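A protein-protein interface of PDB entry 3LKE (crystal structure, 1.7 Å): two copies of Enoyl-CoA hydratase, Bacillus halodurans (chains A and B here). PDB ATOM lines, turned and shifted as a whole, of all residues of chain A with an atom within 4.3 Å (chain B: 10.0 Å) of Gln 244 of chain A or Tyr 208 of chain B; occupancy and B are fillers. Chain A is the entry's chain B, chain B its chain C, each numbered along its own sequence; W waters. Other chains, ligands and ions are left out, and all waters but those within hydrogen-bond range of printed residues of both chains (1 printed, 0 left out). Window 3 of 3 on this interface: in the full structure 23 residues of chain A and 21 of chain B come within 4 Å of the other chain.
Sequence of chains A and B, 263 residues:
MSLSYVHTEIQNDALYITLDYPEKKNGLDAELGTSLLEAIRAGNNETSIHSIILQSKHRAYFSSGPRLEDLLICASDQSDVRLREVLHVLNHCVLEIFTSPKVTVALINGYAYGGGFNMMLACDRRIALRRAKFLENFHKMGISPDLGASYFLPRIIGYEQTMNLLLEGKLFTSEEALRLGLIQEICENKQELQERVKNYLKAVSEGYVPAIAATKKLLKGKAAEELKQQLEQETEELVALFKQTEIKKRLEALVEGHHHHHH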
ATOM      1  N   GLY A 142      -5.799 -24.575  -5.988  1.00  0.00           N
ATOM      2  CA  GLY A 142      -5.413 -24.371  -7.370  1.00  0.00           C
ATOM      3  C   GLY A 142      -6.589 -24.508  -8.327  1.00  0.00           C
ATOM      4  O   GLY A 142      -6.413 -24.857  -9.495  1.00  0.00           O
ATOM      5  N   ALA A 240     -11.463 -27.894 -17.238  1.00  0.00           N
ATOM      6  CA  ALA A 240     -10.188 -27.591 -17.879  1.00  0.00           C
ATOM      7  C   ALA A 240      -9.044 -27.638 -16.870  1.00  0.00           C
ATOM      8  O   ALA A 240      -7.990 -28.204 -17.149  1.00  0.00           O
ATOM      9  CB  ALA A 240     -10.219 -26.245 -18.570  1.00  0.00           C
ATOM     10  N   LEU A 241      -9.248 -27.034 -15.703  1.00  0.00           N
ATOM     11  CA  LEU A 241      -8.210 -27.059 -14.670  1.00  0.00           C
ATOM     12  C   LEU A 241      -7.924 -28.480 -14.165  1.00  0.00           C
ATOM     13  O   LEU A 241      -6.777 -28.810 -13.826  1.00  0.00           O
ATOM     14  CB  LEU A 241      -8.588 -26.131 -13.503  1.00  0.00           C
ATOM     15  CG  LEU A 241      -8.400 -24.642 -13.806  1.00  0.00           C
ATOM     16  CD1 LEU A 241      -9.127 -23.771 -12.771  1.00  0.00           C
ATOM     17  CD2 LEU A 241      -6.913 -24.247 -13.873  1.00  0.00           C
ATOM     18  N   PHE A 242      -8.960 -29.314 -14.114  1.00  0.00           N
ATOM     19  CA  PHE A 242      -8.824 -30.672 -13.580  1.00  0.00           C
ATOM     20  C   PHE A 242      -8.106 -31.611 -14.532  1.00  0.00           C
ATOM     21  O   PHE A 242      -7.821 -32.759 -14.177  1.00  0.00           O
ATOM     22  CB  PHE A 242     -10.176 -31.248 -13.163  1.00  0.00           C
ATOM     23  CG  PHE A 242     -10.504 -31.010 -11.720  1.00  0.00           C
ATOM     24  CD1 PHE A 242     -10.719 -29.722 -11.249  1.00  0.00           C
ATOM     25  CD2 PHE A 242     -10.597 -32.070 -10.832  1.00  0.00           C
ATOM     26  CE1 PHE A 242     -11.019 -29.499  -9.923  1.00  0.00           C
ATOM     27  CE2 PHE A 242     -10.902 -31.857  -9.497  1.00  0.00           C
ATOM     28  CZ  PHE A 242     -11.105 -30.566  -9.038  1.00  0.00           C
ATOM     29  N   LYS A 243      -7.809 -31.117 -15.731  1.00  0.00           N
ATOM     30  CA  LYS A 243      -6.989 -31.862 -16.683  1.00  0.00           C
ATOM     31  C   LYS A 243      -5.516 -31.506 -16.516  1.00  0.00           C
ATOM     32  O   LYS A 243      -4.646 -32.132 -17.130  1.00  0.00           O
ATOM     33  CB  LYS A 243      -7.416 -31.558 -18.125  1.00  0.00           C
ATOM     34  CG  LYS A 243      -8.793 -32.054 -18.506  1.00  0.00           C
ATOM     35  CD  LYS A 243      -9.021 -31.857 -19.999  1.00  0.00           C
ATOM     36  CE  LYS A 243     -10.496 -31.831 -20.340  1.00  0.00           C
ATOM     37  NZ  LYS A 243     -10.733 -31.161 -21.646  1.00  0.00           N
ATOM     38  N   GLN A 244      -5.229 -30.496 -15.693  1.00  0.00           N
ATOM     39  CA  GLN A 244      -3.855 -30.020 -15.510  1.00  0.00           C
ATOM     40  C   GLN A 244      -3.168 -30.676 -14.311  1.00  0.00           C
ATOM     41  O   GLN A 244      -3.741 -30.778 -13.226  1.00  0.00           O
ATOM     42  CB  GLN A 244      -3.819 -28.486 -15.416  1.00  0.00           C
ATOM     43  CG  GLN A 244      -4.320 -27.797 -16.686  1.00  0.00           C
ATOM     44  CD  GLN A 244      -4.331 -26.277 -16.597  1.00  0.00           C
ATOM     45  OE1 GLN A 244      -3.492 -25.672 -15.928  1.00  0.00           O
ATOM     46  NE2 GLN A 244      -5.279 -25.652 -17.290  1.00  0.00           N
ATOM     47  N   THR A 245      -1.930 -31.121 -14.507  1.00  0.00           N
ATOM     48  CA  THR A 245      -1.261 -31.906 -13.477  1.00  0.00           C
ATOM     49  C   THR A 245      -1.203 -31.217 -12.116  1.00  0.00           C
ATOM     50  O   THR A 245      -1.362 -31.871 -11.086  1.00  0.00           O
ATOM     51  CB  THR A 245       0.152 -32.335 -13.910  1.00  0.00           C
ATOM     52  OG1 THR A 245       0.061 -33.053 -15.145  1.00  0.00           O
ATOM     53  CG2 THR A 245       0.763 -33.232 -12.858  1.00  0.00           C
ATOM     54  N   GLU A 246      -1.003 -29.901 -12.111  1.00  0.00           N
ATOM     55  CA  GLU A 246      -0.892 -29.158 -10.861  1.00  0.00           C
ATOM     56  C   GLU A 246      -2.059 -29.445  -9.924  1.00  0.00           C
ATOM     57  O   GLU A 246      -1.873 -29.543  -8.708  1.00  0.00           O
ATOM     58  CB  GLU A 246      -0.801 -27.649 -11.125  1.00  0.00           C
ATOM     59  CG  GLU A 246      -0.649 -26.787  -9.871  1.00  0.00           C
ATOM     60  CD  GLU A 246       0.693 -26.946  -9.164  1.00  0.00           C
ATOM     61  OE1 GLU A 246       1.675 -27.432  -9.779  1.00  0.00           O
ATOM     62  OE2 GLU A 246       0.766 -26.578  -7.976  1.00  0.00           O
ATOM     63  N   ILE A 247      -3.263 -29.550 -10.482  1.00  0.00           N
ATOM     64  CA  ILE A 247      -4.448 -29.765  -9.652  1.00  0.00           C
ATOM     65  C   ILE A 247      -4.422 -31.151  -8.984  1.00  0.00           C
ATOM     66  O   ILE A 247      -4.733 -31.288  -7.797  1.00  0.00           O
ATOM     67  CB  ILE A 247      -5.771 -29.521 -10.428  1.00  0.00           C
ATOM     68  CG1 ILE A 247      -6.015 -28.016 -10.621  1.00  0.00           C
ATOM     69  CG2 ILE A 247      -6.942 -30.097  -9.668  1.00  0.00           C
ATOM     70  CD1 ILE A 247      -4.994 -27.322 -11.478  1.00  0.00           C
ATOM     71  N   LYS A 248      -4.022 -32.164  -9.745  1.00  0.00           N
ATOM     72  CA  LYS A 248      -3.854 -33.515  -9.200  1.00  0.00           C
ATOM     73  C   LYS A 248      -2.847 -33.503  -8.053  1.00  0.00           C
ATOM     74  O   LYS A 248      -3.095 -34.074  -6.987  1.00  0.00           O
ATOM     75  CB  LYS A 248      -3.395 -34.479 -10.298  1.00  0.00           C
ATOM     76  CG  LYS A 248      -3.503 -35.971  -9.934  1.00  0.00           C
ATOM     77  CD  LYS A 248      -2.244 -36.493  -9.278  1.00  0.00           C
ATOM     78  CE  LYS A 248      -1.571 -37.567 -10.136  1.00  0.00           C
ATOM     79  NZ  LYS A 248      -2.447 -38.761 -10.350  1.00  0.00           N
ATOM     80  N   ARG A 250      -1.823 -30.960  -6.104  1.00  0.00           N
ATOM     81  CA  ARG A 250      -2.345 -30.260  -4.934  1.00  0.00           C
ATOM     82  C   ARG A 250      -3.380 -31.075  -4.165  1.00  0.00           C
ATOM     83  O   ARG A 250      -3.420 -31.034  -2.932  1.00  0.00           O
ATOM     84  CB  ARG A 250      -2.921 -28.898  -5.329  1.00  0.00           C
ATOM     85  CG  ARG A 250      -1.863 -27.893  -5.743  1.00  0.00           C
ATOM     86  CD  ARG A 250      -2.469 -26.542  -6.151  1.00  0.00           C
ATOM     87  NE  ARG A 250      -1.410 -25.639  -6.590  1.00  0.00           N
ATOM     88  CZ  ARG A 250      -1.198 -24.415  -6.106  1.00  0.00           C
ATOM     89  NH1 ARG A 250      -2.001 -23.897  -5.177  1.00  0.00           N
ATOM     90  NH2 ARG A 250      -0.188 -23.703  -6.575  1.00  0.00           N
ATOM     91  N   THR B  47       4.173 -15.236 -18.450  1.00  0.00           N
ATOM     92  CA  THR B  47       3.681 -16.431 -17.769  1.00  0.00           C
ATOM     93  C   THR B  47       4.345 -16.653 -16.417  1.00  0.00           C
ATOM     94  O   THR B  47       3.827 -17.386 -15.576  1.00  0.00           O
ATOM     95  CB  THR B  47       3.892 -17.701 -18.621  1.00  0.00           C
ATOM     96  OG1 THR B  47       5.291 -17.852 -18.887  1.00  0.00           O
ATOM     97  CG2 THR B  47       3.144 -17.610 -19.933  1.00  0.00           C
ATOM     98  N   ILE B  49       4.891 -14.515 -13.961  1.00  0.00           N
ATOM     99  CA  ILE B  49       4.443 -13.699 -12.838  1.00  0.00           C
ATOM    100  C   ILE B  49       2.998 -13.993 -12.441  1.00  0.00           C
ATOM    101  O   ILE B  49       2.206 -14.467 -13.257  1.00  0.00           O
ATOM    102  CB  ILE B  49       4.585 -12.183 -13.120  1.00  0.00           C
ATOM    103  CG1 ILE B  49       3.673 -11.749 -14.276  1.00  0.00           C
ATOM    104  CG2 ILE B  49       6.054 -11.812 -13.349  1.00  0.00           C
ATOM    105  CD1 ILE B  49       3.582 -10.212 -14.442  1.00  0.00           C
ATOM    106  N   HIS B  50       2.659 -13.702 -11.187  1.00  0.00           N
ATOM    107  CA  HIS B  50       1.282 -13.869 -10.720  1.00  0.00           C
ATOM    108  C   HIS B  50       0.557 -12.547 -10.463  1.00  0.00           C
ATOM    109  O   HIS B  50      -0.685 -12.519 -10.356  1.00  0.00           O
ATOM    110  CB  HIS B  50       1.237 -14.764  -9.472  1.00  0.00           C
ATOM    111  CG  HIS B  50       2.165 -14.333  -8.374  1.00  0.00           C
ATOM    112  ND1 HIS B  50       2.062 -13.110  -7.746  1.00  0.00           N
ATOM    113  CD2 HIS B  50       3.200 -14.976  -7.781  1.00  0.00           C
ATOM    114  CE1 HIS B  50       2.994 -13.016  -6.814  1.00  0.00           C
ATOM    115  NE2 HIS B  50       3.701 -14.133  -6.816  1.00  0.00           N
ATOM    116  N   SER B  51       1.318 -11.454 -10.367  1.00  0.00           N
ATOM    117  CA  SER B  51       0.752 -10.159  -9.994  1.00  0.00           C
ATOM    118  C   SER B  51       1.380  -8.993 -10.747  1.00  0.00           C
ATOM    119  O   SER B  51       2.520  -9.071 -11.216  1.00  0.00           O
ATOM    120  CB  SER B  51       0.935  -9.916  -8.495  1.00  0.00           C
ATOM    121  OG  SER B  51       0.435 -10.994  -7.736  1.00  0.00           O
ATOM    122  N   PRO B 101      -5.022 -11.065 -16.481  1.00  0.00           N
ATOM    123  CA  PRO B 101      -5.187 -12.351 -15.800  1.00  0.00           C
ATOM    124  C   PRO B 101      -4.393 -12.399 -14.487  1.00  0.00           C
ATOM    125  O   PRO B 101      -4.575 -13.344 -13.715  1.00  0.00           O
ATOM    126  CB  PRO B 101      -4.589 -13.338 -16.793  1.00  0.00           C
ATOM    127  CG  PRO B 101      -3.512 -12.561 -17.471  1.00  0.00           C
ATOM    128  CD  PRO B 101      -4.024 -11.115 -17.561  1.00  0.00           C
ATOM    129  N   LYS B 102      -3.543 -11.402 -14.251  1.00  0.00           N
ATOM    130  CA  LYS B 102      -2.690 -11.355 -13.052  1.00  0.00           C
ATOM    131  C   LYS B 102      -3.430 -10.634 -11.940  1.00  0.00           C
ATOM    132  O   LYS B 102      -4.331  -9.865 -12.209  1.00  0.00           O
ATOM    133  CB  LYS B 102      -1.415 -10.556 -13.338  1.00  0.00           C
ATOM    134  CG  LYS B 102      -0.703 -10.977 -14.616  1.00  0.00           C
ATOM    135  CD  LYS B 102      -0.345 -12.451 -14.581  1.00  0.00           C
ATOM    136  CE  LYS B 102       0.442 -12.843 -15.807  1.00  0.00           C
ATOM    137  NZ  LYS B 102       0.776 -14.316 -15.773  1.00  0.00           N
ATOM    138  N   VAL B 103      -3.040 -10.867 -10.685  1.00  0.00           N
ATOM    139  CA  VAL B 103      -3.620 -10.073  -9.609  1.00  0.00           C
ATOM    140  C   VAL B 103      -3.068  -8.662  -9.730  1.00  0.00           C
ATOM    141  O   VAL B 103      -1.854  -8.460  -9.843  1.00  0.00           O
ATOM    142  CB  VAL B 103      -3.325 -10.674  -8.226  1.00  0.00           C
ATOM    143  CG1 VAL B 103      -3.882  -9.767  -7.115  1.00  0.00           C
ATOM    144  CG2 VAL B 103      -3.889 -12.113  -8.147  1.00  0.00           C
ATOM    145  N   LEU B 201       1.702 -10.414  -1.791  1.00  0.00           N
ATOM    146  CA  LEU B 201       2.270 -11.176  -2.898  1.00  0.00           C
ATOM    147  C   LEU B 201       2.609 -12.618  -2.520  1.00  0.00           C
ATOM    148  O   LEU B 201       2.481 -13.514  -3.345  1.00  0.00           O
ATOM    149  CB  LEU B 201       3.494 -10.462  -3.481  1.00  0.00           C
ATOM    150  CG  LEU B 201       3.229  -9.127  -4.184  1.00  0.00           C
ATOM    151  CD1 LEU B 201       4.520  -8.471  -4.637  1.00  0.00           C
ATOM    152  CD2 LEU B 201       2.280  -9.328  -5.371  1.00  0.00           C
ATOM    153  N   LYS B 202       3.064 -12.842  -1.287  1.00  0.00           N
ATOM    154  CA  LYS B 202       3.272 -14.214  -0.828  1.00  0.00           C
ATOM    155  C   LYS B 202       1.969 -15.005  -0.877  1.00  0.00           C
ATOM    156  O   LYS B 202       1.938 -16.146  -1.346  1.00  0.00           O
ATOM    157  CB  LYS B 202       3.851 -14.252   0.591  1.00  0.00           C
ATOM    158  CG  LYS B 202       4.105 -15.672   1.092  1.00  0.00           C
ATOM    159  CD  LYS B 202       5.085 -16.407   0.195  1.00  0.00           C
ATOM    160  CE  LYS B 202       4.888 -17.925   0.255  1.00  0.00           C
ATOM    161  NZ  LYS B 202       5.002 -18.477   1.638  1.00  0.00           N
ATOM    162  N   ALA B 203       0.897 -14.396  -0.385  1.00  0.00           N
ATOM    163  CA  ALA B 203      -0.411 -15.036  -0.396  1.00  0.00           C
ATOM    164  C   ALA B 203      -0.843 -15.354  -1.827  1.00  0.00           C
ATOM    165  O   ALA B 203      -1.332 -16.446  -2.100  1.00  0.00           O
ATOM    166  CB  ALA B 203      -1.445 -14.167   0.303  1.00  0.00           C
ATOM    167  N   VAL B 204      -0.661 -14.405  -2.739  1.00  0.00           N
ATOM    168  CA  VAL B 204      -0.972 -14.660  -4.143  1.00  0.00           C
ATOM    169  C   VAL B 204      -0.157 -15.831  -4.698  1.00  0.00           C
ATOM    170  O   VAL B 204      -0.689 -16.701  -5.389  1.00  0.00           O
ATOM    171  CB  VAL B 204      -0.752 -13.402  -5.031  1.00  0.00           C
ATOM    172  CG1 VAL B 204      -1.095 -13.717  -6.479  1.00  0.00           C
ATOM    173  CG2 VAL B 204      -1.589 -12.231  -4.526  1.00  0.00           C
ATOM    174  N   SER B 205       1.131 -15.877  -4.359  1.00  0.00           N
ATOM    175  CA  SER B 205       2.031 -16.885  -4.921  1.00  0.00           C
ATOM    176  C   SER B 205       1.670 -18.325  -4.529  1.00  0.00           C
ATOM    177  O   SER B 205       2.066 -19.277  -5.206  1.00  0.00           O
ATOM    178  CB  SER B 205       3.485 -16.594  -4.522  1.00  0.00           C
ATOM    179  OG  SER B 205       3.718 -16.954  -3.170  1.00  0.00           O
ATOM    180  N   GLU B 206       0.927 -18.472  -3.439  1.00  0.00           N
ATOM    181  CA  GLU B 206       0.458 -19.773  -2.958  1.00  0.00           C
ATOM    182  C   GLU B 206      -0.540 -20.399  -3.930  1.00  0.00           C
ATOM    183  O   GLU B 206      -0.831 -21.592  -3.851  1.00  0.00           O
ATOM    184  CB  GLU B 206      -0.254 -19.615  -1.609  1.00  0.00           C
ATOM    185  CG  GLU B 206       0.581 -18.963  -0.505  1.00  0.00           C
ATOM    186  CD  GLU B 206       1.432 -19.963   0.231  1.00  0.00           C
ATOM    187  OE1 GLU B 206       1.262 -21.178  -0.017  1.00  0.00           O
ATOM    188  OE2 GLU B 206       2.267 -19.540   1.059  1.00  0.00           O
ATOM    189  N   GLY B 207      -1.079 -19.583  -4.824  1.00  0.00           N
ATOM    190  CA  GLY B 207      -2.053 -20.062  -5.786  1.00  0.00           C
ATOM    191  C   GLY B 207      -1.432 -20.578  -7.068  1.00  0.00           C
ATOM    192  O   GLY B 207      -0.210 -20.702  -7.191  1.00  0.00           O
ATOM    193  N   TYR B 208      -2.292 -20.882  -8.029  1.00  0.00           N
ATOM    194  CA  TYR B 208      -1.883 -21.432  -9.303  1.00  0.00           C
ATOM    195  C   TYR B 208      -2.289 -20.442 -10.396  1.00  0.00           C
ATOM    196  O   TYR B 208      -3.467 -20.071 -10.514  1.00  0.00           O
ATOM    197  CB  TYR B 208      -2.557 -22.795  -9.500  1.00  0.00           C
ATOM    198  CG  TYR B 208      -2.196 -23.495 -10.793  1.00  0.00           C
ATOM    199  CD1 TYR B 208      -0.869 -23.625 -11.191  1.00  0.00           C
ATOM    200  CD2 TYR B 208      -3.189 -24.025 -11.616  1.00  0.00           C
ATOM    201  CE1 TYR B 208      -0.535 -24.272 -12.384  1.00  0.00           C
ATOM    202  CE2 TYR B 208      -2.861 -24.674 -12.814  1.00  0.00           C
ATOM    203  CZ  TYR B 208      -1.534 -24.786 -13.189  1.00  0.00           C
ATOM    204  OH  TYR B 208      -1.208 -25.436 -14.371  1.00  0.00           O
ATOM    205  N   VAL B 209      -1.313 -20.001 -11.177  1.00  0.00           N
ATOM    206  CA  VAL B 209      -1.529 -18.909 -12.122  1.00  0.00           C
ATOM    207  C   VAL B 209      -2.754 -19.090 -13.054  1.00  0.00           C
ATOM    208  O   VAL B 209      -3.578 -18.186 -13.177  1.00  0.00           O
ATOM    209  CB  VAL B 209      -0.234 -18.544 -12.880  1.00  0.00           C
ATOM    210  CG1 VAL B 209      -0.535 -17.782 -14.170  1.00  0.00           C
ATOM    211  CG2 VAL B 209       0.688 -17.727 -11.980  1.00  0.00           C
ATOM    212  N   PRO B 210      -2.894 -20.262 -13.692  1.00  0.00           N
ATOM    213  CA  PRO B 210      -4.065 -20.447 -14.558  1.00  0.00           C
ATOM    214  C   PRO B 210      -5.392 -20.459 -13.797  1.00  0.00           C
ATOM    215  O   PRO B 210      -6.427 -20.101 -14.372  1.00  0.00           O
ATOM    216  CB  PRO B 210      -3.797 -21.809 -15.220  1.00  0.00           C
ATOM    217  CG  PRO B 210      -2.306 -21.947 -15.181  1.00  0.00           C
ATOM    218  CD  PRO B 210      -1.918 -21.361 -13.855  1.00  0.00           C
ATOM    219  N   ALA B 211      -5.369 -20.873 -12.532  1.00  0.00           N
ATOM    220  CA  ALA B 211      -6.568 -20.871 -11.699  1.00  0.00           C
ATOM    221  C   ALA B 211      -6.978 -19.451 -11.280  1.00  0.00           C
ATOM    222  O   ALA B 211      -8.174 -19.138 -11.221  1.00  0.00           O
ATOM    223  CB  ALA B 211      -6.376 -21.749 -10.465  1.00  0.00           C
ATOM    224  N   ILE B 212      -5.985 -18.616 -10.979  1.00  0.00           N
ATOM    225  CA  ILE B 212      -6.206 -17.193 -10.693  1.00  0.00           C
ATOM    226  C   ILE B 212      -6.850 -16.531 -11.914  1.00  0.00           C
ATOM    227  O   ILE B 212      -7.821 -15.779 -11.795  1.00  0.00           O
ATOM    228  CB  ILE B 212      -4.880 -16.491 -10.362  1.00  0.00           C
ATOM    229  CG1 ILE B 212      -4.357 -16.981  -9.004  1.00  0.00           C
ATOM    230  CG2 ILE B 212      -5.027 -14.979 -10.373  1.00  0.00           C
ATOM    231  CD1 ILE B 212      -2.883 -16.643  -8.745  1.00  0.00           C
ATOM    232  N   ALA B 213      -6.299 -16.828 -13.085  1.00  0.00           N
ATOM    233  CA  ALA B 213      -6.806 -16.252 -14.328  1.00  0.00           C
ATOM    234  C   ALA B 213      -8.247 -16.695 -14.587  1.00  0.00           C
ATOM    235  O   ALA B 213      -9.104 -15.870 -14.950  1.00  0.00           O
ATOM    236  CB  ALA B 213      -5.885 -16.629 -15.499  1.00  0.00           C
ATOM    237  N   ALA B 214      -8.531 -17.977 -14.373  1.00  0.00           N
ATOM    238  CA  ALA B 214      -9.869 -18.504 -14.615  1.00  0.00           C
ATOM    239  C   ALA B 214     -10.829 -17.920 -13.592  1.00  0.00           C
ATOM    240  O   ALA B 214     -11.981 -17.630 -13.897  1.00  0.00           O
ATOM    241  CB  ALA B 214      -9.869 -20.037 -14.540  1.00  0.00           C
ATOM    242  N   THR B 215     -10.337 -17.733 -12.372  1.00  0.00           N
ATOM    243  CA  THR B 215     -11.173 -17.188 -11.313  1.00  0.00           C
ATOM    244  C   THR B 215     -11.622 -15.770 -11.668  1.00  0.00           C
ATOM    245  O   THR B 215     -12.818 -15.430 -11.556  1.00  0.00           O
ATOM    246  CB  THR B 215     -10.418 -17.183  -9.960  1.00  0.00           C
ATOM    247  OG1 THR B 215     -10.177 -18.539  -9.550  1.00  0.00           O
ATOM    248  CG2 THR B 215     -11.257 -16.460  -8.904  1.00  0.00           C
ATOM    249  N   LYS B 216     -10.670 -14.954 -12.104  1.00  0.00           N
ATOM    250  CA  LYS B 216     -10.957 -13.563 -12.476  1.00  0.00           C
ATOM    251  C   LYS B 216     -11.916 -13.500 -13.667  1.00  0.00           C
ATOM    252  O   LYS B 216     -12.846 -12.700 -13.696  1.00  0.00           O
ATOM    253  CB  LYS B 216      -9.666 -12.823 -12.799  1.00  0.00           C
ATOM    254  CG  LYS B 216      -8.830 -12.537 -11.560  1.00  0.00           C
ATOM    255  CD  LYS B 216      -7.662 -11.622 -11.879  1.00  0.00           C
ATOM    256  CE  LYS B 216      -8.121 -10.277 -12.423  1.00  0.00           C
ATOM    257  NZ  LYS B 216      -6.947  -9.378 -12.451  1.00  0.00           N
HETATM  258  O   HOH W   1       2.344 -21.663  -6.363  1.00  0.00           O
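The guanidinium group (NH1) of Arg 250 of chain A is in hydrogen-bond range of the backbone carbonyl oxygen (O) of Glu 206 of chain B.
The side-chain hydroxyl of Tyr 208 of chain B is in hydrogen-bond range of the side-chain amide oxygen of Gln 244 of chain A (2.8 Å).
The guanidinium group (NH2) of Arg 250 of chain A lies within hydrogen-bond range of the backbone carbonyl oxygen (O) of Gly 207 of chain B.
NZ of Lys 202 of chain B lies within salt-bridge range of OE2 of Glu 206 of chain B (3.0 Å).
The backbone carbonyl oxygen (O) of Ala 211 of chain B sits at hydrogen-bond distance from the side-chain hydroxyl (OG1) of Thr 215 of chain B (2.7 Å).
The side-chain carboxylate of Glu 246 of chain A lies within salt-bridge range of the guanidinium group of Arg 250 of chain A, 2.7 Å away.
Among the printed residues, pairs that only touch across the chains: Gly 142 of chain A with Tyr 208 of chain B, Gly 142 of chain A with Ala 211 of chain B, Leu 241 of chain A with Ala 211 of chain B, Gln 244 of chain A with Pro 210 of chain B, Glu 246 of chain A with Tyr 208 of chain B, Ile 247 of chain A with Tyr 208 of chain B and Arg 250 of chain A with Tyr 208 of chain B.
Printed residues of chain B within 4 Å of Leu 241 of chain A: Ala 211 (3.9 Å).
Gln 244 of chain A touches two residues of chain B.
Of the printed residues of chain B, Glu 246 of chain A touches Tyr 208 (3.4 Å).
Printed residues of chain B within 4 Å of Arg 250 of chain A: Glu 206 (2.9 Å), Gly 207 (3.1 Å) and Tyr 208 (3.8 Å).
Pro 101 of chain B touches none of the printed residues of chain A.
Lys 202 of chain B touches none of the printed residues of chain A.
Of the printed residues of chain A, Glu 206 of chain B touches Arg 250 (2.9 Å).
Of chain A, only Gly 142 (3.9 Å), Gln 244 (2.8 Å), Glu 246 (3.4 Å), Ile 247 (3.7 Å) and Arg 250 (3.8 Å) come within 4 Å of Tyr 208 of chain B.
Of the printed residues of chain A, Pro 210 of chain B touches Gln 244.
The nearest residue of chain B that does not touch Gln 244 of chain A is Ala 211 of chain B (6.2 Å).
Of the 23 printed residues of chain B, 5 touch a printed residue of chain A.
Printed residues of chain A that touch a printed residue of chain B: Gly 142, Leu 241, Gln 244, Glu 246, Ile 247 and Arg 250.
Among the printed residues, no Asp or Glu carboxylate lies within 4 Å of a Lys or Arg side-chain nitrogen of the other chain.
No position is printed for both chains.
Water W1 lies within hydrogen-bond range of O of Ser 205 of chain B, O of Gly 207 of chain B and NH2 of Arg 250 of chain A.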
